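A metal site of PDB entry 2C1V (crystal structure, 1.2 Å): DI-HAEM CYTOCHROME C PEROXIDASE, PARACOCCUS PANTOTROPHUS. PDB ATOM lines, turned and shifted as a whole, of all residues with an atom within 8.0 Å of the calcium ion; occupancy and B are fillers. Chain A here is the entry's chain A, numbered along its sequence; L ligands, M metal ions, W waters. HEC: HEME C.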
ATOM      1  N   VAL A  76       6.404   2.066  -7.694  1.00  0.00           N
ATOM      2  CA  VAL A  76       5.064   2.116  -7.123  1.00  0.00           C
ATOM      3  C   VAL A  76       4.048   1.801  -8.175  1.00  0.00           C
ATOM      4  O   VAL A  76       4.397   1.522  -9.319  1.00  0.00           O
ATOM      5  CB  VAL A  76       4.762   3.445  -6.410  1.00  0.00           C
ATOM      6  CG1 VAL A  76       5.821   3.741  -5.320  1.00  0.00           C
ATOM      7  CG2 VAL A  76       4.646   4.615  -7.404  1.00  0.00           C
ATOM      8  N   ASP A  77       2.760   1.829  -7.821  1.00  0.00           N
ATOM      9  CA  ASP A  77       1.729   1.498  -8.787  1.00  0.00           C
ATOM     10  C   ASP A  77       0.957   2.713  -9.290  1.00  0.00           C
ATOM     11  O   ASP A  77       0.218   2.631 -10.263  1.00  0.00           O
ATOM     12  CB  ASP A  77       0.746   0.416  -8.262  1.00  0.00           C
ATOM     13  CG  ASP A  77       0.028   0.796  -7.003  1.00  0.00           C
ATOM     14  OD1 ASP A  77      -0.042   1.970  -6.631  1.00  0.00           O
ATOM     15  OD2 ASP A  77      -0.478  -0.125  -6.292  1.00  0.00           O
ATOM     16  N   GLY A  78       1.170   3.854  -8.645  1.00  0.00           N
ATOM     17  CA  GLY A  78       0.468   5.079  -9.052  1.00  0.00           C
ATOM     18  C   GLY A  78      -1.011   5.122  -8.818  1.00  0.00           C
ATOM     19  O   GLY A  78      -1.713   5.933  -9.425  1.00  0.00           O
ATOM     20  N   LEU A  79      -1.495   4.245  -7.945  1.00  0.00           N
ATOM     21  CA  LEU A  79      -2.910   4.195  -7.560  1.00  0.00           C
ATOM     22  C   LEU A  79      -3.109   4.745  -6.150  1.00  0.00           C
ATOM     23  O   LEU A  79      -2.199   4.695  -5.325  1.00  0.00           O
ATOM     24  CB  LEU A  79      -3.423   2.740  -7.601  1.00  0.00           C
ATOM     25  CG  LEU A  79      -3.195   1.984  -8.907  1.00  0.00           C
ATOM     26  CD1 LEU A  79      -3.773   0.583  -8.786  1.00  0.00           C
ATOM     27  CD2 LEU A  79      -3.791   2.729 -10.091  1.00  0.00           C
ATOM     28  N   PRO A  80      -4.335   5.172  -5.825  1.00  0.00           N
ATOM     29  CA  PRO A  80      -4.640   5.551  -4.415  1.00  0.00           C
ATOM     30  C   PRO A  80      -4.246   4.494  -3.398  1.00  0.00           C
ATOM     31  O   PRO A  80      -3.470   4.751  -2.483  1.00  0.00           O
ATOM     32  CB  PRO A  80      -6.153   5.868  -4.424  1.00  0.00           C
ATOM     33  CG  PRO A  80      -6.359   6.380  -5.827  1.00  0.00           C
ATOM     34  CD  PRO A  80      -5.492   5.467  -6.704  1.00  0.00           C
ATOM     35  N   ASN A  93      -1.662   3.147   0.328  1.00  0.00           N
ATOM     36  CA  ASN A  93      -0.882   3.444  -0.867  1.00  0.00           C
ATOM     37  C   ASN A  93       0.425   2.663  -0.870  1.00  0.00           C
ATOM     38  O   ASN A  93       1.095   2.570   0.154  1.00  0.00           O
ATOM     39  CB  ASN A  93      -0.633   4.960  -0.804  1.00  0.00           C
ATOM     40  CG  ASN A  93       0.049   5.497  -2.052  1.00  0.00           C
ATOM     41  OD1 ASN A  93       1.254   5.788  -2.054  1.00  0.00           O
ATOM     42  ND2 ASN A  93      -0.699   5.588  -3.114  1.00  0.00           N
ATOM     43  N   ALA A  94       0.785   2.109  -2.021  1.00  0.00           N
ATOM     44  CA  ALA A  94       2.040   1.359  -2.110  1.00  0.00           C
ATOM     45  C   ALA A  94       3.237   2.311  -2.131  1.00  0.00           C
ATOM     46  O   ALA A  94       3.333   3.158  -3.022  1.00  0.00           O
ATOM     47  CB  ALA A  94       2.040   0.461  -3.344  1.00  0.00           C
ATOM     48  N   PRO A  95       4.144   2.188  -1.176  1.00  0.00           N
ATOM     49  CA  PRO A  95       5.403   2.984  -1.156  1.00  0.00           C
ATOM     50  C   PRO A  95       6.407   2.332  -2.077  1.00  0.00           C
ATOM     51  O   PRO A  95       6.329   1.163  -2.449  1.00  0.00           O
ATOM     52  CB  PRO A  95       5.883   2.866   0.319  1.00  0.00           C
ATOM     53  CG  PRO A  95       5.366   1.444   0.695  1.00  0.00           C
ATOM     54  CD  PRO A  95       4.077   1.248  -0.025  1.00  0.00           C
ATOM     55  N   THR A  96       7.429   3.093  -2.459  1.00  0.00           N
ATOM     56  CA  THR A  96       8.461   2.569  -3.318  1.00  0.00           C
ATOM     57  C   THR A  96       9.396   1.607  -2.604  1.00  0.00           C
ATOM     58  O   THR A  96       9.711   1.762  -1.433  1.00  0.00           O
ATOM     59  CB  THR A  96       9.267   3.748  -3.932  1.00  0.00           C
ATOM     60  OG1 THR A  96      10.194   3.214  -4.863  1.00  0.00           O
ATOM     61  CG2 THR A  96      10.094   4.560  -2.916  1.00  0.00           C
ATOM     62  N   TRP A 108       4.241   1.515   6.311  1.00  0.00           N
ATOM     63  CA  TRP A 108       3.855   2.819   6.811  1.00  0.00           C
ATOM     64  C   TRP A 108       3.794   2.868   8.344  1.00  0.00           C
ATOM     65  O   TRP A 108       3.838   3.976   8.900  1.00  0.00           O
ATOM     66  CB  TRP A 108       2.470   3.190   6.266  1.00  0.00           C
ATOM     67  CG  TRP A 108       2.438   3.657   4.827  1.00  0.00           C
ATOM     68  CD1 TRP A 108       2.066   2.887   3.753  1.00  0.00           C
ATOM     69  CD2 TRP A 108       2.732   4.960   4.314  1.00  0.00           C
ATOM     70  NE1 TRP A 108       2.137   3.633   2.611  1.00  0.00           N
ATOM     71  CE2 TRP A 108       2.528   4.904   2.920  1.00  0.00           C
ATOM     72  CE3 TRP A 108       3.123   6.177   4.865  1.00  0.00           C
ATOM     73  CZ2 TRP A 108       2.726   5.991   2.071  1.00  0.00           C
ATOM     74  CZ3 TRP A 108       3.299   7.267   4.010  1.00  0.00           C
ATOM     75  CH2 TRP A 108       3.107   7.154   2.658  1.00  0.00           C
ATOM     76  N   ASN A 266      12.649  10.366  -4.506  1.00  0.00           N
ATOM     77  CA  ASN A 266      11.795  10.031  -5.636  1.00  0.00           C
ATOM     78  C   ASN A 266      10.312  10.379  -5.435  1.00  0.00           C
ATOM     79  O   ASN A 266       9.503   9.941  -6.224  1.00  0.00           O
ATOM     80  CB  ASN A 266      11.968   8.576  -6.068  1.00  0.00           C
ATOM     81  CG  ASN A 266      13.426   8.274  -6.364  1.00  0.00           C
ATOM     82  OD1 ASN A 266      13.980   8.817  -7.331  1.00  0.00           O
ATOM     83  ND2 ASN A 266      14.056   7.454  -5.556  1.00  0.00           N
ATOM     84  N   VAL A 267      10.003  11.269  -4.509  1.00  0.00           N
ATOM     85  CA  VAL A 267       8.614  11.597  -4.250  1.00  0.00           C
ATOM     86  C   VAL A 267       7.919  12.165  -5.484  1.00  0.00           C
ATOM     87  O   VAL A 267       6.706  11.970  -5.664  1.00  0.00           O
ATOM     88  CB  VAL A 267       8.460  12.524  -3.036  1.00  0.00           C
ATOM     89  CG1 VAL A 267       9.118  13.937  -3.240  1.00  0.00           C
ATOM     90  CG2 VAL A 267       7.006  12.680  -2.575  1.00  0.00           C
ATOM     91  N   LEU A 269       7.967  11.090  -8.352  1.00  0.00           N
ATOM     92  CA  LEU A 269       7.543   9.993  -9.204  1.00  0.00           C
ATOM     93  C   LEU A 269       6.413   9.151  -8.669  1.00  0.00           C
ATOM     94  O   LEU A 269       5.890   8.286  -9.359  1.00  0.00           O
ATOM     95  CB  LEU A 269       8.707   9.037  -9.429  1.00  0.00           C
ATOM     96  CG  LEU A 269      10.012   9.620  -9.984  1.00  0.00           C
ATOM     97  CD1 LEU A 269      11.067   8.533 -10.190  1.00  0.00           C
ATOM     98  CD2 LEU A 269       9.783  10.357 -11.239  1.00  0.00           C
ATOM     99  N   THR A 270       6.073   9.351  -7.392  1.00  0.00           N
ATOM    100  CA  THR A 270       5.249   8.397  -6.662  1.00  0.00           C
ATOM    101  C   THR A 270       3.916   8.910  -6.182  1.00  0.00           C
ATOM    102  O   THR A 270       3.393   8.424  -5.174  1.00  0.00           O
ATOM    103  CB  THR A 270       6.078   7.765  -5.518  1.00  0.00           C
ATOM    104  OG1 THR A 270       6.427   8.811  -4.601  1.00  0.00           O
ATOM    105  CG2 THR A 270       7.387   7.102  -6.030  1.00  0.00           C
ATOM    106  N   ALA A 271       3.324   9.856  -6.916  1.00  0.00           N
ATOM    107  CA  ALA A 271       1.945  10.244  -6.620  1.00  0.00           C
ATOM    108  C   ALA A 271       1.034   9.027  -6.744  1.00  0.00           C
ATOM    109  O   ALA A 271       1.349   8.036  -7.444  1.00  0.00           O
ATOM    110  CB  ALA A 271       1.509  11.289  -7.609  1.00  0.00           C
ATOM    111  N   PRO A 272      -0.126   9.032  -6.067  1.00  0.00           N
ATOM    112  CA  PRO A 272      -0.594  10.050  -5.098  1.00  0.00           C
ATOM    113  C   PRO A 272       0.056   9.859  -3.735  1.00  0.00           C
ATOM    114  O   PRO A 272       0.833   8.905  -3.506  1.00  0.00           O
ATOM    115  CB  PRO A 272      -2.105   9.788  -5.072  1.00  0.00           C
ATOM    116  CG  PRO A 272      -2.220   8.292  -5.263  1.00  0.00           C
ATOM    117  CD  PRO A 272      -1.090   7.928  -6.206  1.00  0.00           C
ATOM    118  N   TYR A 273      -0.242  10.794  -2.843  1.00  0.00           N
ATOM    119  CA  TYR A 273       0.566  10.978  -1.642  1.00  0.00           C
ATOM    120  C   TYR A 273      -0.157  10.598  -0.356  1.00  0.00           C
ATOM    121  O   TYR A 273      -1.396  10.509  -0.318  1.00  0.00           O
ATOM    122  CB  TYR A 273       1.109  12.426  -1.582  1.00  0.00           C
ATOM    123  CG  TYR A 273       1.951  12.671  -2.811  1.00  0.00           C
ATOM    124  CD1 TYR A 273       3.155  11.974  -2.960  1.00  0.00           C
ATOM    125  CD2 TYR A 273       1.543  13.505  -3.857  1.00  0.00           C
ATOM    126  CE1 TYR A 273       3.942  12.120  -4.094  1.00  0.00           C
ATOM    127  CE2 TYR A 273       2.335  13.672  -4.996  1.00  0.00           C
ATOM    128  CZ  TYR A 273       3.548  12.962  -5.096  1.00  0.00           C
ATOM    129  OH  TYR A 273       4.309  13.130  -6.242  1.00  0.00           O
ATOM    130  N   PHE A 274       0.639  10.424   0.688  1.00  0.00           N
ATOM    131  CA  PHE A 274       0.261   9.931   2.018  1.00  0.00           C
ATOM    132  C   PHE A 274      -0.156   8.475   1.966  1.00  0.00           C
ATOM    133  O   PHE A 274      -0.299   7.891   0.880  1.00  0.00           O
ATOM    134  CB  PHE A 274      -0.775  10.835   2.724  1.00  0.00           C
ATOM    135  CG  PHE A 274      -0.357  12.289   2.766  1.00  0.00           C
ATOM    136  CD1 PHE A 274       0.848  12.647   3.331  1.00  0.00           C
ATOM    137  CD2 PHE A 274      -1.164  13.278   2.241  1.00  0.00           C
ATOM    138  CE1 PHE A 274       1.276  13.995   3.377  1.00  0.00           C
ATOM    139  CE2 PHE A 274      -0.759  14.632   2.291  1.00  0.00           C
ATOM    140  CZ  PHE A 274       0.464  14.969   2.845  1.00  0.00           C
ATOM    141  N   HIS A 275      -0.388   7.871   3.136  1.00  0.00           N
ATOM    142  CA  HIS A 275      -0.746   6.465   3.176  1.00  0.00           C
ATOM    143  C   HIS A 275      -2.096   6.214   2.590  1.00  0.00           C
ATOM    144  O   HIS A 275      -2.410   5.100   2.205  1.00  0.00           O
ATOM    145  CB  HIS A 275      -0.657   5.919   4.598  1.00  0.00           C
ATOM    146  CG  HIS A 275      -1.702   6.463   5.524  1.00  0.00           C
ATOM    147  ND1 HIS A 275      -1.509   7.612   6.236  1.00  0.00           N
ATOM    148  CD2 HIS A 275      -2.932   5.998   5.843  1.00  0.00           C
ATOM    149  CE1 HIS A 275      -2.588   7.848   6.975  1.00  0.00           C
ATOM    150  NE2 HIS A 275      -3.479   6.895   6.717  1.00  0.00           N
ATOM    151  N   SER A 276      -2.912   7.266   2.535  1.00  0.00           N
ATOM    152  CA  SER A 276      -4.278   7.181   2.021  1.00  0.00           C
ATOM    153  C   SER A 276      -4.373   7.396   0.510  1.00  0.00           C
ATOM    154  O   SER A 276      -5.394   7.066  -0.079  1.00  0.00           O
ATOM    155  CB  SER A 276      -5.136   8.219   2.754  1.00  0.00           C
ATOM    156  OG  SER A 276      -4.454   9.451   2.815  1.00  0.00           O
ATOM    157  N   GLY A 277      -3.364   7.975  -0.116  1.00  0.00           N
ATOM    158  CA  GLY A 277      -3.378   8.117  -1.586  1.00  0.00           C
ATOM    159  C   GLY A 277      -4.486   8.975  -2.165  1.00  0.00           C
ATOM    160  O   GLY A 277      -4.906   8.698  -3.298  1.00  0.00           O
ATOM    161  N   VAL A 279      -4.299  12.522  -2.236  1.00  0.00           N
ATOM    162  CA  VAL A 279      -3.722  13.793  -2.648  1.00  0.00           C
ATOM    163  C   VAL A 279      -2.842  13.552  -3.853  1.00  0.00           C
ATOM    164  O   VAL A 279      -1.761  12.966  -3.763  1.00  0.00           O
ATOM    165  CB  VAL A 279      -2.917  14.415  -1.480  1.00  0.00           C
ATOM    166  CG1 VAL A 279      -2.231  15.705  -1.886  1.00  0.00           C
ATOM    167  CG2 VAL A 279      -3.828  14.644  -0.255  1.00  0.00           C
HETATM  168 FE   HEC L   1       6.194  15.215   6.174  1.00  0.00          FE
HETATM  169  CHA HEC L   1       4.707  12.540   4.714  1.00  0.00           C
HETATM  170  CHB HEC L   1       6.557  16.673   3.134  1.00  0.00           C
HETATM  171  CHC HEC L   1       7.167  18.109   7.693  1.00  0.00           C
HETATM  172  CHD HEC L   1       6.147  13.651   9.207  1.00  0.00           C
HETATM  173  NA  HEC L   1       5.772  14.702   4.292  1.00  0.00           N
HETATM  174  C1A HEC L   1       5.113  13.557   3.887  1.00  0.00           C
HETATM  175  C2A HEC L   1       4.832  13.623   2.460  1.00  0.00           C
HETATM  176  C3A HEC L   1       5.379  14.768   1.996  1.00  0.00           C
HETATM  177  C4A HEC L   1       5.939  15.448   3.138  1.00  0.00           C
HETATM  178  CMA HEC L   1       5.399  15.340   0.567  1.00  0.00           C
HETATM  179  CAA HEC L   1       4.147  12.518   1.620  1.00  0.00           C
HETATM  180  CBA HEC L   1       5.203  11.628   0.967  1.00  0.00           C
HETATM  181  CGA HEC L   1       4.629  10.371   0.381  1.00  0.00           C
HETATM  182  O1A HEC L   1       5.440   9.540  -0.117  1.00  0.00           O
HETATM  183  O2A HEC L   1       3.388  10.174   0.366  1.00  0.00           O
HETATM  184  NB  HEC L   1       6.749  17.052   5.557  1.00  0.00           N
HETATM  185  C1B HEC L   1       6.843  17.474   4.233  1.00  0.00           C
HETATM  186  C2B HEC L   1       7.168  18.884   4.196  1.00  0.00           C
HETATM  187  C3B HEC L   1       7.321  19.258   5.478  1.00  0.00           C
HETATM  188  C4B HEC L   1       7.040  18.130   6.334  1.00  0.00           C
HETATM  189  CMB HEC L   1       7.422  19.669   2.908  1.00  0.00           C
HETATM  190  CAB HEC L   1       7.722  20.656   6.005  1.00  0.00           C
HETATM  191  CBB HEC L   1       6.695  21.706   5.501  1.00  0.00           C
HETATM  192  NC  HEC L   1       6.566  15.768   8.109  1.00  0.00           N
HETATM  193  C1C HEC L   1       7.015  17.022   8.510  1.00  0.00           C
HETATM  194  C2C HEC L   1       7.217  17.008   9.925  1.00  0.00           C
HETATM  195  C3C HEC L   1       6.944  15.763  10.371  1.00  0.00           C
HETATM  196  C4C HEC L   1       6.547  14.972   9.202  1.00  0.00           C
HETATM  197  CMC HEC L   1       7.760  18.206  10.760  1.00  0.00           C
HETATM  198  CAC HEC L   1       7.135  15.110  11.730  1.00  0.00           C
HETATM  199  CBC HEC L   1       6.494  15.821  12.911  1.00  0.00           C
HETATM  200  ND  HEC L   1       5.584  13.403   6.837  1.00  0.00           N
HETATM  201  C1D HEC L   1       5.609  12.980   8.131  1.00  0.00           C
HETATM  202  C2D HEC L   1       4.917  11.740   8.264  1.00  0.00           C
HETATM  203  C3D HEC L   1       4.468  11.398   6.920  1.00  0.00           C
HETATM  204  C4D HEC L   1       4.927  12.454   6.071  1.00  0.00           C
HETATM  205  CMD HEC L   1       4.674  10.961   9.530  1.00  0.00           C
HETATM  206  CAD HEC L   1       3.608  10.216   6.528  1.00  0.00           C
HETATM  207  CBD HEC L   1       2.156  10.671   6.819  1.00  0.00           C
HETATM  208  CGD HEC L   1       1.212   9.652   6.273  1.00  0.00           C
HETATM  209  O1D HEC L   1       0.983   9.538   5.063  1.00  0.00           O
HETATM  210  O2D HEC L   1       0.577   8.900   7.117  1.00  0.00           O
HETATM  211 CA    CA M   1       2.590   7.442  -3.146  1.00  0.00          CA
HETATM  212  O   HOH W   1       4.205   5.751  -3.065  1.00  0.00           O
HETATM  213  O   HOH W   2       2.351   8.033  -0.827  1.00  0.00           O
HETATM  214  O   HOH W   3       4.490   8.804  -2.584  1.00  0.00           O
HETATM  215  O   HOH W   4       1.575   6.214  -5.032  1.00  0.00           O
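An oxygen (O2A) of the ligand lies within hydrogen-bond range of the backbone NH (N) of Phe 274 (2.8 Å).
N of His 275 is in hydrogen-bond range of O1D of the ligand (2.9 Å).
A ring nitrogen (ND1) of His 275 is in hydrogen-bond range of an oxygen (O2D) of the ligand.
NE1 of Trp 108 lies within hydrogen-bond range of O of Asn 93, at 2.9 Å.
The side-chain amide nitrogen of Asn 93 lies within hydrogen-bond range of the backbone carbonyl oxygen of Leu 79 (2.8 Å).
The side-chain amide nitrogen (ND2) of Asn 93 lies within hydrogen-bond range of the backbone carbonyl oxygen (O) of Pro 80 (3.0 Å).
The backbone NH (N) of Asn 93 sits at hydrogen-bond distance from the backbone carbonyl oxygen (O) of His 275 (2.8 Å).
The side-chain hydroxyl (OG1) of Thr 270 lies within hydrogen-bond range of the backbone carbonyl oxygen (O) of Val 267.
Within 4 Å of the calcium ion: Asn 93, Thr 270 and Pro 272.
The calcium ion is bound by O of Pro 272 (2.3 Å), water W1 (2.3 Å), OD1 of Asn 93 (2.4 Å), O of Thr 270 (2.4 Å), water W3 (2.4 Å), water W2 (2.4 Å) and water W4 (2.5 Å).
The calcium ion has seven donor atoms within binding distance.
Water W4 bridges O of Ala 271 (3.0 Å) and ND2 of Asn 93 (3.0 Å).
Water W2 bridges O2A of the ligand and O of Phe 274.
Water W3 bridges O1A of the ligand and OG1 of Thr 270.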
